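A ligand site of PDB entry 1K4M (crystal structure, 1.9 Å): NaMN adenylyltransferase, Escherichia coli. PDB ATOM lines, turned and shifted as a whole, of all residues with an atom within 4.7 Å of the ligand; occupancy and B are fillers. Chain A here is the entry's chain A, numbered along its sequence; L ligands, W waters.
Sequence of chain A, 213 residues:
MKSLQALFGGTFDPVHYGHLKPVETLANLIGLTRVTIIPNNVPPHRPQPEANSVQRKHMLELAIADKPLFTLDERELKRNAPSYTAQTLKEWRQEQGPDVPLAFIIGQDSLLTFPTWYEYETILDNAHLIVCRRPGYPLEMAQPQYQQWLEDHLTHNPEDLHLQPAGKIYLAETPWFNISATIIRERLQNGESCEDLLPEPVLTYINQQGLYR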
ATOM      1  N   PHE A   8      -4.156 -20.970   5.730  1.00  0.00           N
ATOM      2  CA  PHE A   8      -3.732 -21.940   6.739  1.00  0.00           C
ATOM      3  C   PHE A   8      -3.302 -23.160   5.954  1.00  0.00           C
ATOM      4  O   PHE A   8      -4.126 -23.826   5.323  1.00  0.00           O
ATOM      5  CB  PHE A   8      -4.955 -22.269   7.619  1.00  0.00           C
ATOM      6  CG  PHE A   8      -4.685 -23.263   8.744  1.00  0.00           C
ATOM      7  CD1 PHE A   8      -5.639 -24.232   9.059  1.00  0.00           C
ATOM      8  CD2 PHE A   8      -3.554 -23.171   9.527  1.00  0.00           C
ATOM      9  CE1 PHE A   8      -5.466 -25.093  10.124  1.00  0.00           C
ATOM     10  CE2 PHE A   8      -3.362 -24.036  10.603  1.00  0.00           C
ATOM     11  CZ  PHE A   8      -4.323 -24.996  10.897  1.00  0.00           C
ATOM     12  N   GLY A   9      -2.017 -23.468   5.966  1.00  0.00           N
ATOM     13  CA  GLY A   9      -1.581 -24.624   5.202  1.00  0.00           C
ATOM     14  C   GLY A   9      -1.311 -25.838   6.046  1.00  0.00           C
ATOM     15  O   GLY A   9      -1.100 -25.735   7.251  1.00  0.00           O
ATOM     16  N   GLY A  10      -1.296 -27.005   5.419  1.00  0.00           N
ATOM     17  CA  GLY A  10      -0.999 -28.214   6.141  1.00  0.00           C
ATOM     18  C   GLY A  10      -1.164 -29.457   5.305  1.00  0.00           C
ATOM     19  O   GLY A  10      -1.599 -29.388   4.147  1.00  0.00           O
ATOM     20  N   THR A  11      -0.783 -30.595   5.884  1.00  0.00           N
ATOM     21  CA  THR A  11      -0.955 -31.887   5.207  1.00  0.00           C
ATOM     22  C   THR A  11      -2.303 -32.492   5.695  1.00  0.00           C
ATOM     23  O   THR A  11      -3.015 -33.107   4.914  1.00  0.00           O
ATOM     24  CB  THR A  11       0.190 -32.829   5.547  1.00  0.00           C
ATOM     25  OG1 THR A  11       1.423 -32.263   5.076  1.00  0.00           O
ATOM     26  CG2 THR A  11      -0.026 -34.169   4.888  1.00  0.00           C
ATOM     27  N   PHE A  12      -2.630 -32.335   6.980  1.00  0.00           N
ATOM     28  CA  PHE A  12      -3.919 -32.835   7.512  1.00  0.00           C
ATOM     29  C   PHE A  12      -4.141 -34.341   7.262  1.00  0.00           C
ATOM     30  O   PHE A  12      -4.992 -34.742   6.461  1.00  0.00           O
ATOM     31  CB  PHE A  12      -5.047 -32.013   6.887  1.00  0.00           C
ATOM     32  CG  PHE A  12      -4.846 -30.523   6.988  1.00  0.00           C
ATOM     33  CD1 PHE A  12      -4.604 -29.745   5.849  1.00  0.00           C
ATOM     34  CD2 PHE A  12      -4.916 -29.876   8.237  1.00  0.00           C
ATOM     35  CE1 PHE A  12      -4.426 -28.344   5.944  1.00  0.00           C
ATOM     36  CE2 PHE A  12      -4.741 -28.483   8.343  1.00  0.00           C
ATOM     37  CZ  PHE A  12      -4.501 -27.714   7.206  1.00  0.00           C
ATOM     38  N   HIS A  16      -8.022 -32.454  12.119  1.00  0.00           N
ATOM     39  CA  HIS A  16      -8.604 -32.704  13.436  1.00  0.00           C
ATOM     40  C   HIS A  16      -8.815 -31.399  14.206  1.00  0.00           C
ATOM     41  O   HIS A  16      -8.495 -30.303  13.717  1.00  0.00           O
ATOM     42  CB  HIS A  16      -7.713 -33.655  14.234  1.00  0.00           C
ATOM     43  CG  HIS A  16      -6.351 -33.107  14.503  1.00  0.00           C
ATOM     44  ND1 HIS A  16      -5.195 -33.677  13.998  1.00  0.00           N
ATOM     45  CD2 HIS A  16      -5.955 -32.019  15.207  1.00  0.00           C
ATOM     46  CE1 HIS A  16      -4.156 -32.971  14.378  1.00  0.00           C
ATOM     47  NE2 HIS A  16      -4.581 -31.967  15.124  1.00  0.00           N
ATOM     48  N   GLY A  18      -7.274 -30.066  16.671  1.00  0.00           N
ATOM     49  CA  GLY A  18      -6.059 -29.326  16.973  1.00  0.00           C
ATOM     50  C   GLY A  18      -5.692 -28.395  15.821  1.00  0.00           C
ATOM     51  O   GLY A  18      -4.969 -27.416  16.053  1.00  0.00           O
ATOM     52  N   HIS A  19      -6.173 -28.698  14.607  1.00  0.00           N
ATOM     53  CA  HIS A  19      -5.929 -27.841  13.437  1.00  0.00           C
ATOM     54  C   HIS A  19      -7.016 -26.765  13.390  1.00  0.00           C
ATOM     55  O   HIS A  19      -6.736 -25.586  13.243  1.00  0.00           O
ATOM     56  CB  HIS A  19      -6.042 -28.600  12.084  1.00  0.00           C
ATOM     57  CG  HIS A  19      -5.160 -29.806  11.940  1.00  0.00           C
ATOM     58  ND1 HIS A  19      -3.788 -29.768  12.112  1.00  0.00           N
ATOM     59  CD2 HIS A  19      -5.451 -31.079  11.585  1.00  0.00           C
ATOM     60  CE1 HIS A  19      -3.273 -30.961  11.868  1.00  0.00           C
ATOM     61  NE2 HIS A  19      -4.270 -31.775  11.544  1.00  0.00           N
ATOM     62  N   PRO A  22      -8.176 -23.973  17.094  1.00  0.00           N
ATOM     63  CA  PRO A  22      -7.368 -22.786  17.396  1.00  0.00           C
ATOM     64  C   PRO A  22      -7.674 -21.686  16.357  1.00  0.00           C
ATOM     65  O   PRO A  22      -7.824 -20.511  16.720  1.00  0.00           O
ATOM     66  CB  PRO A  22      -5.934 -23.322  17.278  1.00  0.00           C
ATOM     67  CG  PRO A  22      -6.079 -24.774  17.736  1.00  0.00           C
ATOM     68  CD  PRO A  22      -7.349 -25.187  17.002  1.00  0.00           C
ATOM     69  N   ILE A  38      -5.036 -24.483   2.791  1.00  0.00           N
ATOM     70  CA  ILE A  38      -4.253 -24.893   1.631  1.00  0.00           C
ATOM     71  C   ILE A  38      -3.587 -26.243   1.874  1.00  0.00           C
ATOM     72  O   ILE A  38      -2.471 -26.312   2.398  1.00  0.00           O
ATOM     73  CB  ILE A  38      -3.164 -23.848   1.293  1.00  0.00           C
ATOM     74  CG1 ILE A  38      -3.812 -22.463   1.105  1.00  0.00           C
ATOM     75  CG2 ILE A  38      -2.392 -24.270   0.033  1.00  0.00           C
ATOM     76  CD1 ILE A  38      -2.826 -21.339   0.757  1.00  0.00           C
ATOM     77  N   ASN A  40      -1.553 -29.699   1.120  1.00  0.00           N
ATOM     78  CA  ASN A  40      -0.480 -30.047   0.199  1.00  0.00           C
ATOM     79  C   ASN A  40      -0.421 -31.549  -0.065  1.00  0.00           C
ATOM     80  O   ASN A  40      -1.047 -32.339   0.645  1.00  0.00           O
ATOM     81  CB  ASN A  40       0.883 -29.511   0.672  1.00  0.00           C
ATOM     82  CG  ASN A  40       1.254 -29.942   2.096  1.00  0.00           C
ATOM     83  OD1 ASN A  40       0.960 -31.064   2.528  1.00  0.00           O
ATOM     84  ND2 ASN A  40       1.937 -29.057   2.817  1.00  0.00           N
ATOM     85  N   HIS A  45       9.633 -31.740   3.699  1.00  0.00           N
ATOM     86  CA  HIS A  45       9.996 -31.701   5.104  1.00  0.00           C
ATOM     87  C   HIS A  45       9.393 -32.812   5.952  1.00  0.00           C
ATOM     88  O   HIS A  45       9.505 -32.763   7.177  1.00  0.00           O
ATOM     89  CB  HIS A  45       9.584 -30.354   5.718  1.00  0.00           C
ATOM     90  CG  HIS A  45       8.109 -30.229   5.958  1.00  0.00           C
ATOM     91  ND1 HIS A  45       7.202 -30.052   4.931  1.00  0.00           N
ATOM     92  CD2 HIS A  45       7.391 -30.268   7.104  1.00  0.00           C
ATOM     93  CE1 HIS A  45       5.985 -29.978   5.438  1.00  0.00           C
ATOM     94  NE2 HIS A  45       6.067 -30.106   6.750  1.00  0.00           N
ATOM     95  N   ARG A  46       8.764 -33.792   5.325  1.00  0.00           N
ATOM     96  CA  ARG A  46       8.154 -34.859   6.106  1.00  0.00           C
ATOM     97  C   ARG A  46       7.867 -36.129   5.296  1.00  0.00           C
ATOM     98  O   ARG A  46       7.788 -36.092   4.078  1.00  0.00           O
ATOM     99  CB  ARG A  46       6.855 -34.341   6.771  1.00  0.00           C
ATOM    100  CG  ARG A  46       5.819 -33.753   5.806  1.00  0.00           C
ATOM    101  CD  ARG A  46       4.645 -33.179   6.582  1.00  0.00           C
ATOM    102  NE  ARG A  46       3.674 -34.204   6.987  1.00  0.00           N
ATOM    103  CZ  ARG A  46       2.758 -34.040   7.943  1.00  0.00           C
ATOM    104  NH1 ARG A  46       2.672 -32.898   8.624  1.00  0.00           N
ATOM    105  NH2 ARG A  46       1.898 -35.015   8.187  1.00  0.00           N
ATOM    106  N   GLU A  76      -2.023 -26.258  -4.287  1.00  0.00           N
ATOM    107  CA  GLU A  76      -0.881 -27.100  -3.983  1.00  0.00           C
ATOM    108  C   GLU A  76      -1.149 -28.587  -4.255  1.00  0.00           C
ATOM    109  O   GLU A  76      -0.220 -29.359  -4.495  1.00  0.00           O
ATOM    110  CB  GLU A  76      -0.392 -26.861  -2.547  1.00  0.00           C
ATOM    111  CG  GLU A  76       0.169 -25.444  -2.348  1.00  0.00           C
ATOM    112  CD  GLU A  76       0.865 -25.256  -1.019  1.00  0.00           C
ATOM    113  OE1 GLU A  76       0.873 -26.214  -0.200  1.00  0.00           O
ATOM    114  OE2 GLU A  76       1.416 -24.146  -0.784  1.00  0.00           O
ATOM    115  N   TYR A  84       5.993 -24.776  -2.296  1.00  0.00           N
ATOM    116  CA  TYR A  84       6.728 -24.125  -1.228  1.00  0.00           C
ATOM    117  C   TYR A  84       5.870 -22.954  -0.785  1.00  0.00           C
ATOM    118  O   TYR A  84       5.377 -22.179  -1.612  1.00  0.00           O
ATOM    119  CB  TYR A  84       8.088 -23.628  -1.720  1.00  0.00           C
ATOM    120  CG  TYR A  84       8.937 -24.731  -2.284  1.00  0.00           C
ATOM    121  CD1 TYR A  84       8.867 -25.062  -3.639  1.00  0.00           C
ATOM    122  CD2 TYR A  84       9.770 -25.472  -1.455  1.00  0.00           C
ATOM    123  CE1 TYR A  84       9.615 -26.110  -4.159  1.00  0.00           C
ATOM    124  CE2 TYR A  84      10.526 -26.531  -1.964  1.00  0.00           C
ATOM    125  CZ  TYR A  84      10.441 -26.837  -3.313  1.00  0.00           C
ATOM    126  OH  TYR A  84      11.188 -27.893  -3.821  1.00  0.00           O
ATOM    127  N   THR A  85       5.706 -22.807   0.519  1.00  0.00           N
ATOM    128  CA  THR A  85       4.860 -21.734   1.027  1.00  0.00           C
ATOM    129  C   THR A  85       5.314 -20.374   0.518  1.00  0.00           C
ATOM    130  O   THR A  85       4.497 -19.517   0.207  1.00  0.00           O
ATOM    131  CB  THR A  85       4.872 -21.719   2.541  1.00  0.00           C
ATOM    132  OG1 THR A  85       4.519 -23.017   3.019  1.00  0.00           O
ATOM    133  CG2 THR A  85       3.864 -20.673   3.064  1.00  0.00           C
ATOM    134  N   ALA A  86       6.622 -20.176   0.454  1.00  0.00           N
ATOM    135  CA  ALA A  86       7.116 -18.895  -0.023  1.00  0.00           C
ATOM    136  C   ALA A  86       6.537 -18.655  -1.428  1.00  0.00           C
ATOM    137  O   ALA A  86       6.162 -17.546  -1.769  1.00  0.00           O
ATOM    138  CB  ALA A  86       8.644 -18.876  -0.042  1.00  0.00           C
ATOM    139  N   PHE A 104      -0.530 -15.771   7.117  1.00  0.00           N
ATOM    140  CA  PHE A 104      -0.376 -17.217   6.975  1.00  0.00           C
ATOM    141  C   PHE A 104      -0.322 -17.749   8.408  1.00  0.00           C
ATOM    142  O   PHE A 104       0.517 -17.353   9.220  1.00  0.00           O
ATOM    143  CB  PHE A 104       0.909 -17.569   6.205  1.00  0.00           C
ATOM    144  CG  PHE A 104       1.044 -19.065   5.909  1.00  0.00           C
ATOM    145  CD1 PHE A 104       0.304 -19.653   4.902  1.00  0.00           C
ATOM    146  CD2 PHE A 104       1.868 -19.883   6.699  1.00  0.00           C
ATOM    147  CE1 PHE A 104       0.368 -21.019   4.648  1.00  0.00           C
ATOM    148  CE2 PHE A 104       1.944 -21.281   6.460  1.00  0.00           C
ATOM    149  CZ  PHE A 104       1.180 -21.846   5.429  1.00  0.00           C
ATOM    150  N   ILE A 105      -1.231 -18.666   8.735  1.00  0.00           N
ATOM    151  CA  ILE A 105      -1.341 -19.200  10.069  1.00  0.00           C
ATOM    152  C   ILE A 105      -0.592 -20.511  10.305  1.00  0.00           C
ATOM    153  O   ILE A 105      -0.748 -21.444   9.535  1.00  0.00           O
ATOM    154  CB  ILE A 105      -2.824 -19.475  10.418  1.00  0.00           C
ATOM    155  CG1 ILE A 105      -3.670 -18.211  10.251  1.00  0.00           C
ATOM    156  CG2 ILE A 105      -2.921 -19.989  11.840  1.00  0.00           C
ATOM    157  CD1 ILE A 105      -5.196 -18.501  10.148  1.00  0.00           C
ATOM    158  N   ILE A 106       0.174 -20.587  11.400  1.00  0.00           N
ATOM    159  CA  ILE A 106       0.891 -21.813  11.725  1.00  0.00           C
ATOM    160  C   ILE A 106       0.819 -22.112  13.226  1.00  0.00           C
ATOM    161  O   ILE A 106       0.376 -21.286  14.008  1.00  0.00           O
ATOM    162  CB  ILE A 106       2.402 -21.709  11.330  1.00  0.00           C
ATOM    163  CG1 ILE A 106       3.081 -20.598  12.149  1.00  0.00           C
ATOM    164  CG2 ILE A 106       2.532 -21.422   9.861  1.00  0.00           C
ATOM    165  CD1 ILE A 106       4.503 -20.288  11.714  1.00  0.00           C
ATOM    166  N   GLY A 107       1.232 -23.307  13.621  1.00  0.00           N
ATOM    167  CA  GLY A 107       1.233 -23.651  15.026  1.00  0.00           C
ATOM    168  C   GLY A 107       2.607 -23.334  15.592  1.00  0.00           C
ATOM    169  O   GLY A 107       3.592 -23.180  14.851  1.00  0.00           O
ATOM    170  N   ASP A 109       4.746 -25.136  16.897  1.00  0.00           N
ATOM    171  CA  ASP A 109       5.774 -26.098  16.482  1.00  0.00           C
ATOM    172  C   ASP A 109       6.335 -25.778  15.105  1.00  0.00           C
ATOM    173  O   ASP A 109       7.509 -26.066  14.832  1.00  0.00           O
ATOM    174  CB  ASP A 109       5.223 -27.531  16.467  1.00  0.00           C
ATOM    175  CG  ASP A 109       4.127 -27.712  15.434  1.00  0.00           C
ATOM    176  OD1 ASP A 109       3.102 -27.010  15.523  1.00  0.00           O
ATOM    177  OD2 ASP A 109       4.283 -28.541  14.524  1.00  0.00           O
ATOM    178  N   SER A 110       5.545 -25.191  14.228  1.00  0.00           N
ATOM    179  CA  SER A 110       6.068 -24.855  12.889  1.00  0.00           C
ATOM    180  C   SER A 110       6.871 -23.557  12.951  1.00  0.00           C
ATOM    181  O   SER A 110       7.794 -23.370  12.176  1.00  0.00           O
ATOM    182  CB  SER A 110       4.928 -24.738  11.872  1.00  0.00           C
ATOM    183  OG  SER A 110       4.256 -25.978  11.739  1.00  0.00           O
ATOM    184  N   TRP A 117      12.620 -23.245   6.263  1.00  0.00           N
ATOM    185  CA  TRP A 117      11.727 -23.300   5.108  1.00  0.00           C
ATOM    186  C   TRP A 117      12.340 -22.663   3.845  1.00  0.00           C
ATOM    187  O   TRP A 117      13.171 -21.759   3.914  1.00  0.00           O
ATOM    188  CB  TRP A 117      10.400 -22.578   5.409  1.00  0.00           C
ATOM    189  CG  TRP A 117       9.502 -23.230   6.405  1.00  0.00           C
ATOM    190  CD1 TRP A 117       9.846 -24.116   7.402  1.00  0.00           C
ATOM    191  CD2 TRP A 117       8.112 -22.948   6.590  1.00  0.00           C
ATOM    192  NE1 TRP A 117       8.754 -24.390   8.192  1.00  0.00           N
ATOM    193  CE2 TRP A 117       7.673 -23.685   7.715  1.00  0.00           C
ATOM    194  CE3 TRP A 117       7.189 -22.137   5.914  1.00  0.00           C
ATOM    195  CZ2 TRP A 117       6.358 -23.633   8.176  1.00  0.00           C
ATOM    196  CZ3 TRP A 117       5.893 -22.091   6.376  1.00  0.00           C
ATOM    197  CH2 TRP A 117       5.484 -22.837   7.491  1.00  0.00           C
ATOM    198  N   TYR A 118      11.904 -23.137   2.686  1.00  0.00           N
ATOM    199  CA  TYR A 118      12.380 -22.625   1.392  1.00  0.00           C
ATOM    200  C   TYR A 118      12.180 -21.106   1.301  1.00  0.00           C
ATOM    201  O   TYR A 118      11.062 -20.625   1.424  1.00  0.00           O
ATOM    202  CB  TYR A 118      11.584 -23.315   0.300  1.00  0.00           C
ATOM    203  CG  TYR A 118      11.877 -22.838  -1.078  1.00  0.00           C
ATOM    204  CD1 TYR A 118      13.005 -23.261  -1.766  1.00  0.00           C
ATOM    205  CD2 TYR A 118      11.019 -21.934  -1.708  1.00  0.00           C
ATOM    206  CE1 TYR A 118      13.282 -22.797  -3.050  1.00  0.00           C
ATOM    207  CE2 TYR A 118      11.276 -21.465  -2.993  1.00  0.00           C
ATOM    208  CZ  TYR A 118      12.410 -21.905  -3.648  1.00  0.00           C
ATOM    209  OH  TYR A 118      12.689 -21.428  -4.914  1.00  0.00           O
ATOM    210  N   ARG A 133      -0.866 -21.091  19.654  1.00  0.00           N
ATOM    211  CA  ARG A 133      -0.202 -21.780  20.739  1.00  0.00           C
ATOM    212  C   ARG A 133      -0.376 -23.279  20.690  1.00  0.00           C
ATOM    213  O   ARG A 133      -1.416 -23.797  20.302  1.00  0.00           O
ATOM    214  CB  ARG A 133      -0.761 -21.287  22.088  1.00  0.00           C
ATOM    215  CG  ARG A 133      -0.564 -19.796  22.330  1.00  0.00           C
ATOM    216  CD  ARG A 133      -0.965 -19.400  23.742  1.00  0.00           C
ATOM    217  NE  ARG A 133      -2.418 -19.466  23.939  1.00  0.00           N
ATOM    218  CZ  ARG A 133      -3.040 -18.785  24.896  1.00  0.00           C
ATOM    219  NH1 ARG A 133      -2.351 -18.021  25.726  1.00  0.00           N
ATOM    220  NH2 ARG A 133      -4.367 -18.855  25.012  1.00  0.00           N
ATOM    221  N   ARG A 134       0.653 -23.990  21.108  1.00  0.00           N
ATOM    222  CA  ARG A 134       0.576 -25.428  21.159  1.00  0.00           C
ATOM    223  C   ARG A 134       1.212 -25.768  22.487  1.00  0.00           C
ATOM    224  O   ARG A 134       2.322 -25.346  22.786  1.00  0.00           O
ATOM    225  CB  ARG A 134       1.329 -26.030  19.987  1.00  0.00           C
ATOM    226  CG  ARG A 134       0.956 -27.476  19.800  1.00  0.00           C
ATOM    227  CD  ARG A 134       1.352 -27.999  18.438  1.00  0.00           C
ATOM    228  NE  ARG A 134       1.007 -29.403  18.366  1.00  0.00           N
ATOM    229  CZ  ARG A 134       1.253 -30.182  17.326  1.00  0.00           C
ATOM    230  NH1 ARG A 134       1.861 -29.695  16.236  1.00  0.00           N
ATOM    231  NH2 ARG A 134       0.907 -31.462  17.377  1.00  0.00           N
ATOM    232  N   PHE A 177      -4.487 -27.651  22.593  1.00  0.00           N
ATOM    233  CA  PHE A 177      -4.997 -28.991  22.372  1.00  0.00           C
ATOM    234  C   PHE A 177      -3.869 -30.010  22.247  1.00  0.00           C
ATOM    235  O   PHE A 177      -3.014 -29.896  21.352  1.00  0.00           O
ATOM    236  CB  PHE A 177      -5.862 -29.072  21.099  1.00  0.00           C
ATOM    237  CG  PHE A 177      -7.091 -28.210  21.116  1.00  0.00           C
ATOM    238  CD1 PHE A 177      -7.069 -26.914  20.580  1.00  0.00           C
ATOM    239  CD2 PHE A 177      -8.293 -28.690  21.655  1.00  0.00           C
ATOM    240  CE1 PHE A 177      -8.210 -26.109  20.585  1.00  0.00           C
ATOM    241  CE2 PHE A 177      -9.455 -27.888  21.670  1.00  0.00           C
ATOM    242  CZ  PHE A 177      -9.414 -26.598  21.135  1.00  0.00           C
ATOM    243  N   ILE A 179      -3.428 -32.613  20.788  1.00  0.00           N
ATOM    244  CA  ILE A 179      -3.934 -33.493  19.730  1.00  0.00           C
ATOM    245  C   ILE A 179      -2.972 -33.434  18.529  1.00  0.00           C
ATOM    246  O   ILE A 179      -2.468 -32.367  18.184  1.00  0.00           O
ATOM    247  CB  ILE A 179      -5.358 -33.054  19.296  1.00  0.00           C
ATOM    248  CG1 ILE A 179      -6.350 -33.267  20.460  1.00  0.00           C
ATOM    249  CG2 ILE A 179      -5.814 -33.811  18.028  1.00  0.00           C
ATOM    250  CD1 ILE A 179      -7.599 -32.496  20.319  1.00  0.00           C
HETATM  251  P1  LIG L   1       0.259 -30.134   9.586  1.00  0.00           P
HETATM  252  O1  LIG L   1      -0.803 -30.739   8.787  1.00  0.00           O
HETATM  253  O2  LIG L   1       0.999 -31.063  10.463  1.00  0.00           O
HETATM  254  O3  LIG L   1      -0.364 -29.026  10.591  1.00  0.00           O
HETATM  255  C1  LIG L   1      -1.153 -27.941  10.035  1.00  0.00           C
HETATM  256  C2  LIG L   1      -0.901 -26.747  10.978  1.00  0.00           C
HETATM  257  O4  LIG L   1      -1.516 -26.928  12.275  1.00  0.00           O
HETATM  258  C3  LIG L   1       0.570 -26.444  11.281  1.00  0.00           C
HETATM  259  O5  LIG L   1       0.795 -25.005  11.157  1.00  0.00           O
HETATM  260  C4  LIG L   1       0.715 -26.983  12.694  1.00  0.00           C
HETATM  261  O6  LIG L   1       1.761 -26.297  13.370  1.00  0.00           O
HETATM  262  C5  LIG L   1      -0.654 -26.692  13.322  1.00  0.00           C
HETATM  263  N1  LIG L   1      -1.032 -27.637  14.356  1.00  0.00           N
HETATM  264  C6  LIG L   1      -1.015 -29.007  14.265  1.00  0.00           C
HETATM  265  N2  LIG L   1      -1.419 -29.618  15.390  1.00  0.00           N
HETATM  266  C7  LIG L   1      -1.713 -28.539  16.245  1.00  0.00           C
HETATM  267  C8  LIG L   1      -2.197 -28.499  17.579  1.00  0.00           C
HETATM  268  N3  LIG L   1      -2.466 -29.574  18.296  1.00  0.00           N
HETATM  269  N4  LIG L   1      -2.388 -27.260  18.156  1.00  0.00           N
HETATM  270  C9  LIG L   1      -2.116 -26.137  17.411  1.00  0.00           C
HETATM  271  N5  LIG L   1      -1.654 -26.097  16.146  1.00  0.00           N
HETATM  272  C10 LIG L   1      -1.482 -27.324  15.618  1.00  0.00           C
HETATM  273  O7  LIG L   1       1.230 -29.370   8.563  1.00  0.00           O
HETATM  274  P2  LIG L   1       2.807 -29.072   8.744  1.00  0.00           P
HETATM  275  O8  LIG L   1       3.693 -30.178   8.292  1.00  0.00           O
HETATM  276  O9  LIG L   1       3.078 -28.681  10.160  1.00  0.00           O
HETATM  277  O10 LIG L   1       2.935 -27.865   7.665  1.00  0.00           O
HETATM  278  C11 LIG L   1       2.218 -26.613   7.932  1.00  0.00           C
HETATM  279  C12 LIG L   1       2.477 -25.694   6.783  1.00  0.00           C
HETATM  280  O11 LIG L   1       3.876 -25.275   6.747  1.00  0.00           O
HETATM  281  C13 LIG L   1       2.138 -26.261   5.394  1.00  0.00           C
HETATM  282  O12 LIG L   1       1.472 -25.280   4.579  1.00  0.00           O
HETATM  283  C14 LIG L   1       3.514 -26.595   4.843  1.00  0.00           C
HETATM  284  O13 LIG L   1       3.551 -26.654   3.405  1.00  0.00           O
HETATM  285  C15 LIG L   1       4.363 -25.495   5.409  1.00  0.00           C
HETATM  286  N6  LIG L   1       5.803 -25.808   5.390  1.00  0.00           N
HETATM  287  C16 LIG L   1       6.565 -25.286   4.324  1.00  0.00           C
HETATM  288  C17 LIG L   1       7.995 -25.529   4.193  1.00  0.00           C
HETATM  289  C18 LIG L   1       8.647 -24.890   3.010  1.00  0.00           C
HETATM  290  O14 LIG L   1       9.867 -25.099   2.937  1.00  0.00           O
HETATM  291  N7  LIG L   1       7.983 -24.145   2.098  1.00  0.00           N
HETATM  292  C19 LIG L   1       8.672 -26.366   5.219  1.00  0.00           C
HETATM  293  C20 LIG L   1       7.782 -26.897   6.338  1.00  0.00           C
HETATM  294  C21 LIG L   1       6.478 -26.619   6.372  1.00  0.00           C
HETATM  295  O   HOH W   1       8.658 -21.774   1.538  1.00  0.00           O
HETATM  296  O   HOH W   2       0.115 -25.795   2.314  1.00  0.00           O
HETATM  297  O   HOH W   3       3.505 -27.273   0.677  1.00  0.00           O
HETATM  298  O   HOH W   4       0.054 -23.822   8.766  1.00  0.00           O
HETATM  299  O   HOH W   5      10.970 -27.326   2.466  1.00  0.00           O
HETATM  300  O   HOH W   6       2.022 -23.455   1.837  1.00  0.00           O
HETATM  301  O   HOH W   7      -0.249 -30.595  20.618  1.00  0.00           O
HETATM  302  O   HOH W   8       2.881 -29.887   5.417  1.00  0.00           O
HETATM  303  O   HOH W   9       2.946 -29.572  12.487  1.00  0.00           O
HETATM  304  O   HOH W  10       8.616 -28.773   2.705  1.00  0.00           O
HETATM  305  O   HOH W  11      -1.941 -23.730  14.445  1.00  0.00           O
HETATM  306  O   HOH W  12      -2.810 -26.258  20.560  1.00  0.00           O
HETATM  307  O   HOH W  13      11.473 -27.427   7.015  1.00  0.00           O
HETATM  308  O   HOH W  14      -1.274 -32.321  14.606  1.00  0.00           O
HETATM  309  O   HOH W  15      -0.939 -32.666  11.671  1.00  0.00           O
HETATM  310  O   HOH W  16       5.948 -27.848   2.192  1.00  0.00           O
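Water W12 lies within hydrogen-bond range of a nitrogen (N4) of the ligand, the backbone carbonyl oxygen of Arg 133 and the backbone NH of Phe 177.
Water W2 lies within hydrogen-bond range of O of Ile 38 (2.6 Å), OE1 of Glu 76 (2.7 Å) and O12 of the ligand (2.7 Å).
Water W4 lies within hydrogen-bond range of O of Ile 105, O of Gly 9 and O5 of the ligand.
Water W14 bridges N2 of the ligand (2.8 Å) and NE2 of His 16 (3.4 Å).
Water W11 lies within hydrogen-bond range of N5 of the ligand, N of Gly 107 and O of Ile 106.
Water W8 lies within hydrogen-bond range of the side-chain hydroxyl (OG1) of Thr 11 (2.8 Å), the side-chain amide nitrogen (ND2) of Asn 40 (2.9 Å), an oxygen (O8) of the ligand (3.0 Å) and a ring nitrogen (NE2) of His 45 (3.5 Å).
N4 of the ligand lies close to O of Gly 18 (3.3 Å).
The backbone NH (N) of Thr 85 lies close to a nitrogen (N7) of the ligand (3.1 Å).
Phe 8 touches the ligand.
Gly 9 touches the ligand.
His 16 touches the ligand.
ND1 of His 19 touches C6 of the ligand, 3.6 Å away.
CA of Tyr 84 touches N7 of the ligand, 3.6 Å away.
Phe 104 touches the ligand.
Ile 106 touches the ligand (CA to O5, 3.2 Å).
Trp 117 touches the ligand.
Arg 133 touches the ligand.
Hydrophobic or aromatic side chains within 4 Å of the ligand: Phe 8, His 19, His 45, Tyr 84, Phe 104, Ile 106, Trp 117 and Tyr 118.
Within 4 Å of the ligand: Phe 8, Gly 9, Gly 10, Thr 11, Phe 12, His 16, Gly 18, His 19, Asn 40, His 45, Arg 46, Tyr 84, Thr 85, Phe 104, Ile 106, Gly 107, Asp 109, Ser 110, Trp 117, Tyr 118, Arg 133, Arg 134, Phe 177 and Ile 179.
The nearest printed residue that does not touch the ligand is Pro 22 (4.2 Å).
NH1 of Arg 134 lies within salt-bridge range of OD1 of Asp 109, 3.0 Å away.
The side-chain hydroxyl (OG1) of Thr 11 is in hydrogen-bond range of the side-chain amide oxygen (OD1) of Asn 40 (2.9 Å).
O of Gly 10 lies within hydrogen-bond range of N of Asn 40 (3.0 Å).
The backbone NH (N) of Gly 10 is in hydrogen-bond range of the backbone carbonyl oxygen (O) of Ile 38, 3.3 Å away.
NE2 of His 19 lies close to ND1 of His 16 (3.2 Å).
The backbone carbonyl oxygen of Phe 8 sits at hydrogen-bond distance from the backbone NH of Ile 38 (2.8 Å).
The side-chain carboxylate (OD1) of Asp 109 lies within hydrogen-bond range of an oxygen (O6) of the ligand (2.6 Å).
A nitrogen (N3) of the ligand is in hydrogen-bond range of the backbone carbonyl oxygen (O) of Ile 179 (2.8 Å).
An oxygen (O8) of the ligand is in hydrogen-bond range of a ring nitrogen (NE2) of His 45 (2.8 Å).
An oxygen (O14) of the ligand is in hydrogen-bond range of the backbone NH of Tyr 118 (2.8 Å).
The backbone NH (N) of Thr 11 sits at hydrogen-bond distance from an oxygen (O1) of the ligand (2.9 Å).
O8 of the ligand is in salt-bridge range of NH1 of Arg 46 (2.9 Å).
ND2 of Asn 40 sits at hydrogen-bond distance from O13 of the ligand (3.0 Å).
The side-chain hydroxyl (OG) of Ser 110 is in hydrogen-bond range of an oxygen (O6) of the ligand (3.0 Å).
An oxygen (O5) of the ligand lies within hydrogen-bond range of the backbone NH of Gly 107.
N of Phe 12 lies within hydrogen-bond range of O1 of the ligand (3.0 Å).
O of Phe 177 lies within hydrogen-bond range of N3 of the ligand (3.1 Å).
The guanidinium group of Arg 134 sits close to a nitrogen (N2) of the ligand.
An oxygen (O12) of the ligand lies within hydrogen-bond range of the backbone NH (N) of Gly 10, at 3.4 Å.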
